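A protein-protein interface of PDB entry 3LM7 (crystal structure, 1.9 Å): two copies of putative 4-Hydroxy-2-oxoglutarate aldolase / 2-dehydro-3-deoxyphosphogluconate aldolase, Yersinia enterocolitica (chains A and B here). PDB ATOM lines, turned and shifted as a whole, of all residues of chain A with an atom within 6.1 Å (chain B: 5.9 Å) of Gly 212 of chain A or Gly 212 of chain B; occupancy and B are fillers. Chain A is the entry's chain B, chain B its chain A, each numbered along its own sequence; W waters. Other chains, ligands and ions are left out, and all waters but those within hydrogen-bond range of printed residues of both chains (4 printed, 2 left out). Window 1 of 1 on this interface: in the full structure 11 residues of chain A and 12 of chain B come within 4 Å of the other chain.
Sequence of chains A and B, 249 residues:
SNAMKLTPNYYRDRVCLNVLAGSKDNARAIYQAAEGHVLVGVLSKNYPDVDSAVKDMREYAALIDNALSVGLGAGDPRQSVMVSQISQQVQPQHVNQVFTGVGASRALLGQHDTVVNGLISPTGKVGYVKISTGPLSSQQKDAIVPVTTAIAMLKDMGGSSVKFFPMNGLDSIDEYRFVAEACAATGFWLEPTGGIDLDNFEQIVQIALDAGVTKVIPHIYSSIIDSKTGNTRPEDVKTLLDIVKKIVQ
The backbone carbonyl oxygen (O) of Ala 185 of chain B lies within hydrogen-bond range of the guanidinium group (NH1) of Arg 14 of chain A. The backbone carbonyl oxygen (O) of Ala 184 of chain B lies within hydrogen-bond range of the guanidinium group (NH2) of Arg 14 of chain A, at 3.3 Å. O of Leu 209 of chain A sits close to O of Ala 185 of chain B (3.2 Å).
The guanidinium group (NH2) of Arg 14 of chain A sits at hydrogen-bond distance from the backbone carbonyl oxygen (O) of Leu 209 of chain A (3.0 Å). The backbone carbonyl oxygen (O) of Val 213 of chain A is in hydrogen-bond range of the guanidinium group (NH2) of Arg 14 of chain A (2.9 Å). NE of Arg 14 of chain B is in hydrogen-bond range of O of Thr 214 of chain B, 3.3 Å away.
O of Ala 184 of chain A touches O of Leu 209 of chain B, at 3.8 Å. Ala 184 of chain A touches Gly 212 of chain B (O to CA, 3.3 Å). Ala 185 of chain A touches Leu 209 of chain B. O of Asp 210 of chain B touches CB of Ala 185 of chain A, at 3.4 Å. Leu 209 of chain A touches Ala 184 of chain B. Ala 185 of chain B touches Asp 210 of chain A. Ala 211 of chain A touches Ala 211 of chain B. Gly 212 of chain A touches Ala 184 of chain B. Gly 212 of chain A touches Gly 212 of chain B (O to O, 3.6 Å). Thr 214 of chain B touches Thr 214 of chain A.
Cys 183 of chain A touches none of the printed residues of chain B. Printed residues of chain B within 4 Å of Ala 185 of chain A: Leu 209 and Asp 210. Ile 207 of chain A touches none of the printed residues of chain B. Of the printed residues of chain B, Ala 211 of chain A touches Ala 211 (3.9 Å). Of the printed residues of chain B, Gly 212 of chain A touches Ala 184 and Gly 212. Of the printed residues of chain A, Ala 185 of chain B touches Arg 14, Leu 209 and Asp 210. Gly 212 of chain B touches just these residues of chain A: Ala 184 and Gly 212. The nearest printed residue of chain A that does not touch Ala 185 of chain B is Gly 212 of chain A (4.3 Å).
Of the 13 printed residues of chain B, 7 touch a printed residue of chain A. Of the 13 printed residues of chain A, 8 touch a printed residue of chain B. Hydrophobic or aromatic side chains of chain A within 4 Å of the printed part of chain B: Ala 185. Among the printed residues, 13 pairs touch across the chains.
Arg 14 of chain A touches Ala 184 of chain B, but with the chains exchanged Ala 184 of chain A does not touch Arg 14 of chain B (4.6 Å). Ala 185 of chain A touches Leu 209 of chain B, and with the chains exchanged Leu 209 of chain A touches Ala 185 of chain B. Ala 185 of chain A touches Asp 210 of chain B, and with the chains exchanged Asp 210 of chain A touches Ala 185 of chain B. Thr 214 of chain B touches its own counterpart, Thr 214 of chain A.
Water W4 lies within hydrogen-bond range of OD1 of Asp 210 of chain B and O of Ala 185 of chain A. Water W2 bridges the backbone carbonyl oxygen of Ala 185 of chain B and the side-chain carboxylate of Asp 210 of chain A. Water W1 lies within hydrogen-bond range of the side-chain hydroxyl of Thr 214 of chain A and the guanidinium group of Arg 14 of chain B. Water W3 lies within hydrogen-bond range of O of Asp 210 of chain A (2.8 Å) and O of Glu 181 of chain B (2.8 Å).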
ATOM      1  N   ARG A  14      -1.741 -21.594 -22.607  1.00  0.00           N
ATOM      2  CA  ARG A  14      -2.574 -21.874 -21.456  1.00  0.00           C
ATOM      3  C   ARG A  14      -4.057 -22.139 -21.868  1.00  0.00           C
ATOM      4  O   ARG A  14      -4.708 -22.988 -21.270  1.00  0.00           O
ATOM      5  CB  ARG A  14      -2.507 -20.628 -20.534  1.00  0.00           C
ATOM      6  CG  ARG A  14      -3.002 -20.800 -19.081  1.00  0.00           C
ATOM      7  CD  ARG A  14      -1.861 -21.381 -18.150  1.00  0.00           C
ATOM      8  NE  ARG A  14      -2.408 -21.915 -16.888  1.00  0.00           N
ATOM      9  CZ  ARG A  14      -2.537 -21.279 -15.737  1.00  0.00           C
ATOM     10  NH1 ARG A  14      -2.154 -20.001 -15.583  1.00  0.00           N
ATOM     11  NH2 ARG A  14      -3.030 -21.957 -14.708  1.00  0.00           N
ATOM     12  N   ALA A 180     -10.639 -29.063 -11.000  1.00  0.00           N
ATOM     13  CA  ALA A 180      -9.534 -28.252 -11.515  1.00  0.00           C
ATOM     14  C   ALA A 180      -8.289 -28.426 -10.594  1.00  0.00           C
ATOM     15  O   ALA A 180      -7.166 -28.565 -11.073  1.00  0.00           O
ATOM     16  CB  ALA A 180      -9.979 -26.779 -11.535  1.00  0.00           C
ATOM     17  N   CYS A 183      -6.796 -31.768 -11.383  1.00  0.00           N
ATOM     18  CA  CYS A 183      -6.078 -31.670 -12.660  1.00  0.00           C
ATOM     19  C   CYS A 183      -4.704 -30.987 -12.511  1.00  0.00           C
ATOM     20  O   CYS A 183      -3.689 -31.479 -12.998  1.00  0.00           O
ATOM     21  CB  CYS A 183      -6.911 -30.904 -13.667  1.00  0.00           C
ATOM     22  SG  CYS A 183      -8.330 -31.949 -14.316  1.00  0.00           S
ATOM     23  N   ALA A 184      -4.673 -29.900 -11.773  1.00  0.00           N
ATOM     24  CA  ALA A 184      -3.374 -29.178 -11.591  1.00  0.00           C
ATOM     25  C   ALA A 184      -2.330 -30.107 -10.949  1.00  0.00           C
ATOM     26  O   ALA A 184      -1.183 -30.175 -11.374  1.00  0.00           O
ATOM     27  CB  ALA A 184      -3.602 -28.012 -10.715  1.00  0.00           C
ATOM     28  N   ALA A 185      -2.777 -30.852  -9.932  1.00  0.00           N
ATOM     29  CA  ALA A 185      -1.889 -31.763  -9.165  1.00  0.00           C
ATOM     30  C   ALA A 185      -1.428 -32.964  -9.935  1.00  0.00           C
ATOM     31  O   ALA A 185      -0.503 -33.638  -9.504  1.00  0.00           O
ATOM     32  CB  ALA A 185      -2.537 -32.182  -7.853  1.00  0.00           C
ATOM     33  N   ILE A 207     -11.258 -19.783 -12.522  1.00  0.00           N
ATOM     34  CA  ILE A 207     -11.175 -20.844 -11.457  1.00  0.00           C
ATOM     35  C   ILE A 207     -10.087 -21.928 -11.851  1.00  0.00           C
ATOM     36  O   ILE A 207      -9.271 -22.380 -10.997  1.00  0.00           O
ATOM     37  CB  ILE A 207     -12.544 -21.529 -11.272  1.00  0.00           C
ATOM     38  CG1 ILE A 207     -13.460 -20.565 -10.453  1.00  0.00           C
ATOM     39  CG2 ILE A 207     -12.423 -22.912 -10.535  1.00  0.00           C
ATOM     40  CD1 ILE A 207     -14.908 -21.076 -10.458  1.00  0.00           C
ATOM     41  N   ALA A 208     -10.105 -22.321 -13.112  1.00  0.00           N
ATOM     42  CA  ALA A 208      -9.114 -23.321 -13.607  1.00  0.00           C
ATOM     43  C   ALA A 208      -7.704 -22.768 -13.567  1.00  0.00           C
ATOM     44  O   ALA A 208      -6.774 -23.454 -13.155  1.00  0.00           O
ATOM     45  CB  ALA A 208      -9.448 -23.778 -15.078  1.00  0.00           C
ATOM     46  N   LEU A 209      -7.533 -21.523 -14.020  1.00  0.00           N
ATOM     47  CA  LEU A 209      -6.240 -20.857 -13.955  1.00  0.00           C
ATOM     48  C   LEU A 209      -5.679 -20.767 -12.524  1.00  0.00           C
ATOM     49  O   LEU A 209      -4.485 -21.102 -12.286  1.00  0.00           O
ATOM     50  CB  LEU A 209      -6.338 -19.457 -14.629  1.00  0.00           C
ATOM     51  CG  LEU A 209      -6.723 -19.416 -16.087  1.00  0.00           C
ATOM     52  CD1 LEU A 209      -6.803 -17.962 -16.462  1.00  0.00           C
ATOM     53  CD2 LEU A 209      -5.648 -20.167 -16.958  1.00  0.00           C
ATOM     54  N   ASP A 210      -6.502 -20.307 -11.586  1.00  0.00           N
ATOM     55  CA  ASP A 210      -6.092 -20.124 -10.185  1.00  0.00           C
ATOM     56  C   ASP A 210      -5.810 -21.443  -9.522  1.00  0.00           C
ATOM     57  O   ASP A 210      -4.954 -21.489  -8.609  1.00  0.00           O
ATOM     58  CB  ASP A 210      -7.174 -19.399  -9.357  1.00  0.00           C
ATOM     59  CG  ASP A 210      -7.349 -17.944  -9.742  1.00  0.00           C
ATOM     60  OD1 ASP A 210      -6.537 -17.416 -10.510  1.00  0.00           O
ATOM     61  OD2 ASP A 210      -8.358 -17.346  -9.266  1.00  0.00           O
ATOM     62  N   ALA A 211      -6.482 -22.521  -9.960  1.00  0.00           N
ATOM     63  CA  ALA A 211      -6.228 -23.847  -9.401  1.00  0.00           C
ATOM     64  C   ALA A 211      -4.874 -24.381  -9.902  1.00  0.00           C
ATOM     65  O   ALA A 211      -4.387 -25.381  -9.378  1.00  0.00           O
ATOM     66  CB  ALA A 211      -7.310 -24.855  -9.858  1.00  0.00           C
ATOM     67  N   GLY A 212      -4.372 -23.834 -10.989  1.00  0.00           N
ATOM     68  CA  GLY A 212      -3.059 -24.283 -11.504  1.00  0.00           C
ATOM     69  C   GLY A 212      -3.159 -25.232 -12.670  1.00  0.00           C
ATOM     70  O   GLY A 212      -2.145 -25.846 -13.065  1.00  0.00           O
ATOM     71  N   VAL A 213      -4.321 -25.275 -13.331  1.00  0.00           N
ATOM     72  CA  VAL A 213      -4.457 -26.097 -14.526  1.00  0.00           C
ATOM     73  C   VAL A 213      -3.553 -25.625 -15.672  1.00  0.00           C
ATOM     74  O   VAL A 213      -3.576 -24.439 -16.068  1.00  0.00           O
ATOM     75  CB  VAL A 213      -5.961 -26.271 -14.971  1.00  0.00           C
ATOM     76  CG1 VAL A 213      -6.023 -27.193 -16.168  1.00  0.00           C
ATOM     77  CG2 VAL A 213      -6.816 -26.867 -13.839  1.00  0.00           C
ATOM     78  N   THR A 214      -2.741 -26.537 -16.209  1.00  0.00           N
ATOM     79  CA  THR A 214      -1.794 -26.148 -17.283  1.00  0.00           C
ATOM     80  C   THR A 214      -2.461 -25.657 -18.577  1.00  0.00           C
ATOM     81  O   THR A 214      -2.089 -24.585 -19.139  1.00  0.00           O
ATOM     82  CB  THR A 214      -0.865 -27.365 -17.586  1.00  0.00           C
ATOM     83  OG1 THR A 214      -0.170 -27.661 -16.385  1.00  0.00           O
ATOM     84  CG2 THR A 214       0.148 -27.127 -18.786  1.00  0.00           C
ATOM     85  N   ARG B  14       8.143 -31.743 -17.608  1.00  0.00           N
ATOM     86  CA  ARG B  14       7.818 -31.199 -16.289  1.00  0.00           C
ATOM     87  C   ARG B  14       9.027 -30.794 -15.487  1.00  0.00           C
ATOM     88  O   ARG B  14       8.998 -29.744 -14.860  1.00  0.00           O
ATOM     89  CB  ARG B  14       6.996 -32.176 -15.438  1.00  0.00           C
ATOM     90  CG  ARG B  14       5.564 -32.441 -15.870  1.00  0.00           C
ATOM     91  CD  ARG B  14       4.642 -31.189 -15.776  1.00  0.00           C
ATOM     92  NE  ARG B  14       4.365 -30.535 -14.471  1.00  0.00           N
ATOM     93  CZ  ARG B  14       3.500 -30.965 -13.555  1.00  0.00           C
ATOM     94  NH1 ARG B  14       2.923 -32.157 -13.707  1.00  0.00           N
ATOM     95  NH2 ARG B  14       3.261 -30.264 -12.432  1.00  0.00           N
ATOM     96  N   ALA B 180       4.989 -21.789  -4.883  1.00  0.00           N
ATOM     97  CA  ALA B 180       4.599 -22.837  -5.817  1.00  0.00           C
ATOM     98  C   ALA B 180       3.141 -22.673  -6.275  1.00  0.00           C
ATOM     99  O   ALA B 180       2.838 -22.747  -7.485  1.00  0.00           O
ATOM    100  CB  ALA B 180       4.859 -24.227  -5.183  1.00  0.00           C
ATOM    101  N   GLU B 181       2.225 -22.398  -5.340  1.00  0.00           N
ATOM    102  CA  GLU B 181       0.788 -22.220  -5.733  1.00  0.00           C
ATOM    103  C   GLU B 181       0.577 -20.981  -6.600  1.00  0.00           C
ATOM    104  O   GLU B 181      -0.184 -21.032  -7.582  1.00  0.00           O
ATOM    105  CB  GLU B 181      -0.101 -22.159  -4.496  1.00  0.00           C
ATOM    106  CG  GLU B 181       0.369 -23.210  -3.556  1.00  0.00           C
ATOM    107  CD  GLU B 181      -0.650 -24.131  -3.132  1.00  0.00           C
ATOM    108  OE1 GLU B 181      -1.232 -24.720  -4.113  1.00  0.00           O
ATOM    109  OE2 GLU B 181      -0.823 -24.288  -1.850  1.00  0.00           O
ATOM    110  N   ALA B 184       1.979 -21.796 -10.154  1.00  0.00           N
ATOM    111  CA  ALA B 184       0.968 -22.623 -10.853  1.00  0.00           C
ATOM    112  C   ALA B 184      -0.170 -21.716 -11.304  1.00  0.00           C
ATOM    113  O   ALA B 184      -0.649 -21.823 -12.447  1.00  0.00           O
ATOM    114  CB  ALA B 184       0.432 -23.747  -9.894  1.00  0.00           C
ATOM    115  N   ALA B 185      -0.639 -20.858 -10.407  1.00  0.00           N
ATOM    116  CA  ALA B 185      -1.794 -19.976 -10.783  1.00  0.00           C
ATOM    117  C   ALA B 185      -1.478 -19.083 -11.992  1.00  0.00           C
ATOM    118  O   ALA B 185      -2.357 -18.783 -12.813  1.00  0.00           O
ATOM    119  CB  ALA B 185      -2.200 -19.073  -9.562  1.00  0.00           C
ATOM    120  N   ILE B 207       6.084 -30.999  -3.751  1.00  0.00           N
ATOM    121  CA  ILE B 207       5.289 -29.807  -3.403  1.00  0.00           C
ATOM    122  C   ILE B 207       4.983 -28.964  -4.624  1.00  0.00           C
ATOM    123  O   ILE B 207       3.852 -28.496  -4.816  1.00  0.00           O
ATOM    124  CB  ILE B 207       6.074 -28.969  -2.358  1.00  0.00           C
ATOM    125  CG1 ILE B 207       5.890 -29.614  -0.996  1.00  0.00           C
ATOM    126  CG2 ILE B 207       5.611 -27.469  -2.348  1.00  0.00           C
ATOM    127  CD1 ILE B 207       6.914 -29.055   0.034  1.00  0.00           C
ATOM    128  N   ALA B 208       5.992 -28.764  -5.475  1.00  0.00           N
ATOM    129  CA  ALA B 208       5.796 -27.964  -6.713  1.00  0.00           C
ATOM    130  C   ALA B 208       4.844 -28.687  -7.675  1.00  0.00           C
ATOM    131  O   ALA B 208       3.976 -28.027  -8.305  1.00  0.00           O
ATOM    132  CB  ALA B 208       7.185 -27.673  -7.467  1.00  0.00           C
ATOM    133  N   LEU B 209       5.009 -30.011  -7.829  1.00  0.00           N
ATOM    134  CA  LEU B 209       4.115 -30.741  -8.720  1.00  0.00           C
ATOM    135  C   LEU B 209       2.677 -30.733  -8.199  1.00  0.00           C
ATOM    136  O   LEU B 209       1.753 -30.562  -8.989  1.00  0.00           O
ATOM    137  CB  LEU B 209       4.577 -32.206  -8.885  1.00  0.00           C
ATOM    138  CG  LEU B 209       5.972 -32.407  -9.477  1.00  0.00           C
ATOM    139  CD1 LEU B 209       6.362 -33.951  -9.469  1.00  0.00           C
ATOM    140  CD2 LEU B 209       6.033 -31.845 -10.954  1.00  0.00           C
ATOM    141  N   ASP B 210       2.479 -30.888  -6.879  1.00  0.00           N
ATOM    142  CA  ASP B 210       1.103 -30.915  -6.324  1.00  0.00           C
ATOM    143  C   ASP B 210       0.419 -29.543  -6.454  1.00  0.00           C
ATOM    144  O   ASP B 210      -0.784 -29.518  -6.657  1.00  0.00           O
ATOM    145  CB  ASP B 210       1.085 -31.299  -4.838  1.00  0.00           C
ATOM    146  CG  ASP B 210       1.410 -32.794  -4.597  1.00  0.00           C
ATOM    147  OD1 ASP B 210       1.488 -33.593  -5.562  1.00  0.00           O
ATOM    148  OD2 ASP B 210       1.611 -33.139  -3.426  1.00  0.00           O
ATOM    149  N   ALA B 211       1.203 -28.450  -6.360  1.00  0.00           N
ATOM    150  CA  ALA B 211       0.703 -27.080  -6.647  1.00  0.00           C
ATOM    151  C   ALA B 211       0.285 -26.886  -8.111  1.00  0.00           C
ATOM    152  O   ALA B 211      -0.667 -26.106  -8.409  1.00  0.00           O
ATOM    153  CB  ALA B 211       1.773 -26.018  -6.230  1.00  0.00           C
ATOM    154  N   GLY B 212       0.905 -27.634  -9.018  1.00  0.00           N
ATOM    155  CA  GLY B 212       0.550 -27.579 -10.443  1.00  0.00           C
ATOM    156  C   GLY B 212       1.604 -26.788 -11.255  1.00  0.00           C
ATOM    157  O   GLY B 212       1.358 -26.400 -12.401  1.00  0.00           O
ATOM    158  N   VAL B 213       2.785 -26.548 -10.669  1.00  0.00           N
ATOM    159  CA  VAL B 213       3.827 -25.837 -11.421  1.00  0.00           C
ATOM    160  C   VAL B 213       4.206 -26.608 -12.725  1.00  0.00           C
ATOM    161  O   VAL B 213       4.547 -27.782 -12.656  1.00  0.00           O
ATOM    162  CB  VAL B 213       5.094 -25.542 -10.581  1.00  0.00           C
ATOM    163  CG1 VAL B 213       6.109 -24.737 -11.391  1.00  0.00           C
ATOM    164  CG2 VAL B 213       4.711 -24.796  -9.295  1.00  0.00           C
ATOM    165  N   THR B 214       4.146 -25.923 -13.861  1.00  0.00           N
ATOM    166  CA  THR B 214       4.319 -26.530 -15.170  1.00  0.00           C
ATOM    167  C   THR B 214       5.757 -27.018 -15.446  1.00  0.00           C
ATOM    168  O   THR B 214       5.932 -28.115 -16.022  1.00  0.00           O
ATOM    169  CB  THR B 214       3.863 -25.568 -16.247  1.00  0.00           C
ATOM    170  OG1 THR B 214       2.474 -25.287 -15.954  1.00  0.00           O
ATOM    171  CG2 THR B 214       3.869 -26.275 -17.610  1.00  0.00           C
HETATM  172  O   HOH W   1       1.837 -29.491 -16.339  1.00  0.00           O
HETATM  173  O   HOH W   2      -4.342 -17.140 -12.317  1.00  0.00           O
HETATM  174  O   HOH W   3      -2.524 -22.610  -7.838  1.00  0.00           O
HETATM  175  O   HOH W   4      -0.336 -35.112  -6.429  1.00  0.00           O
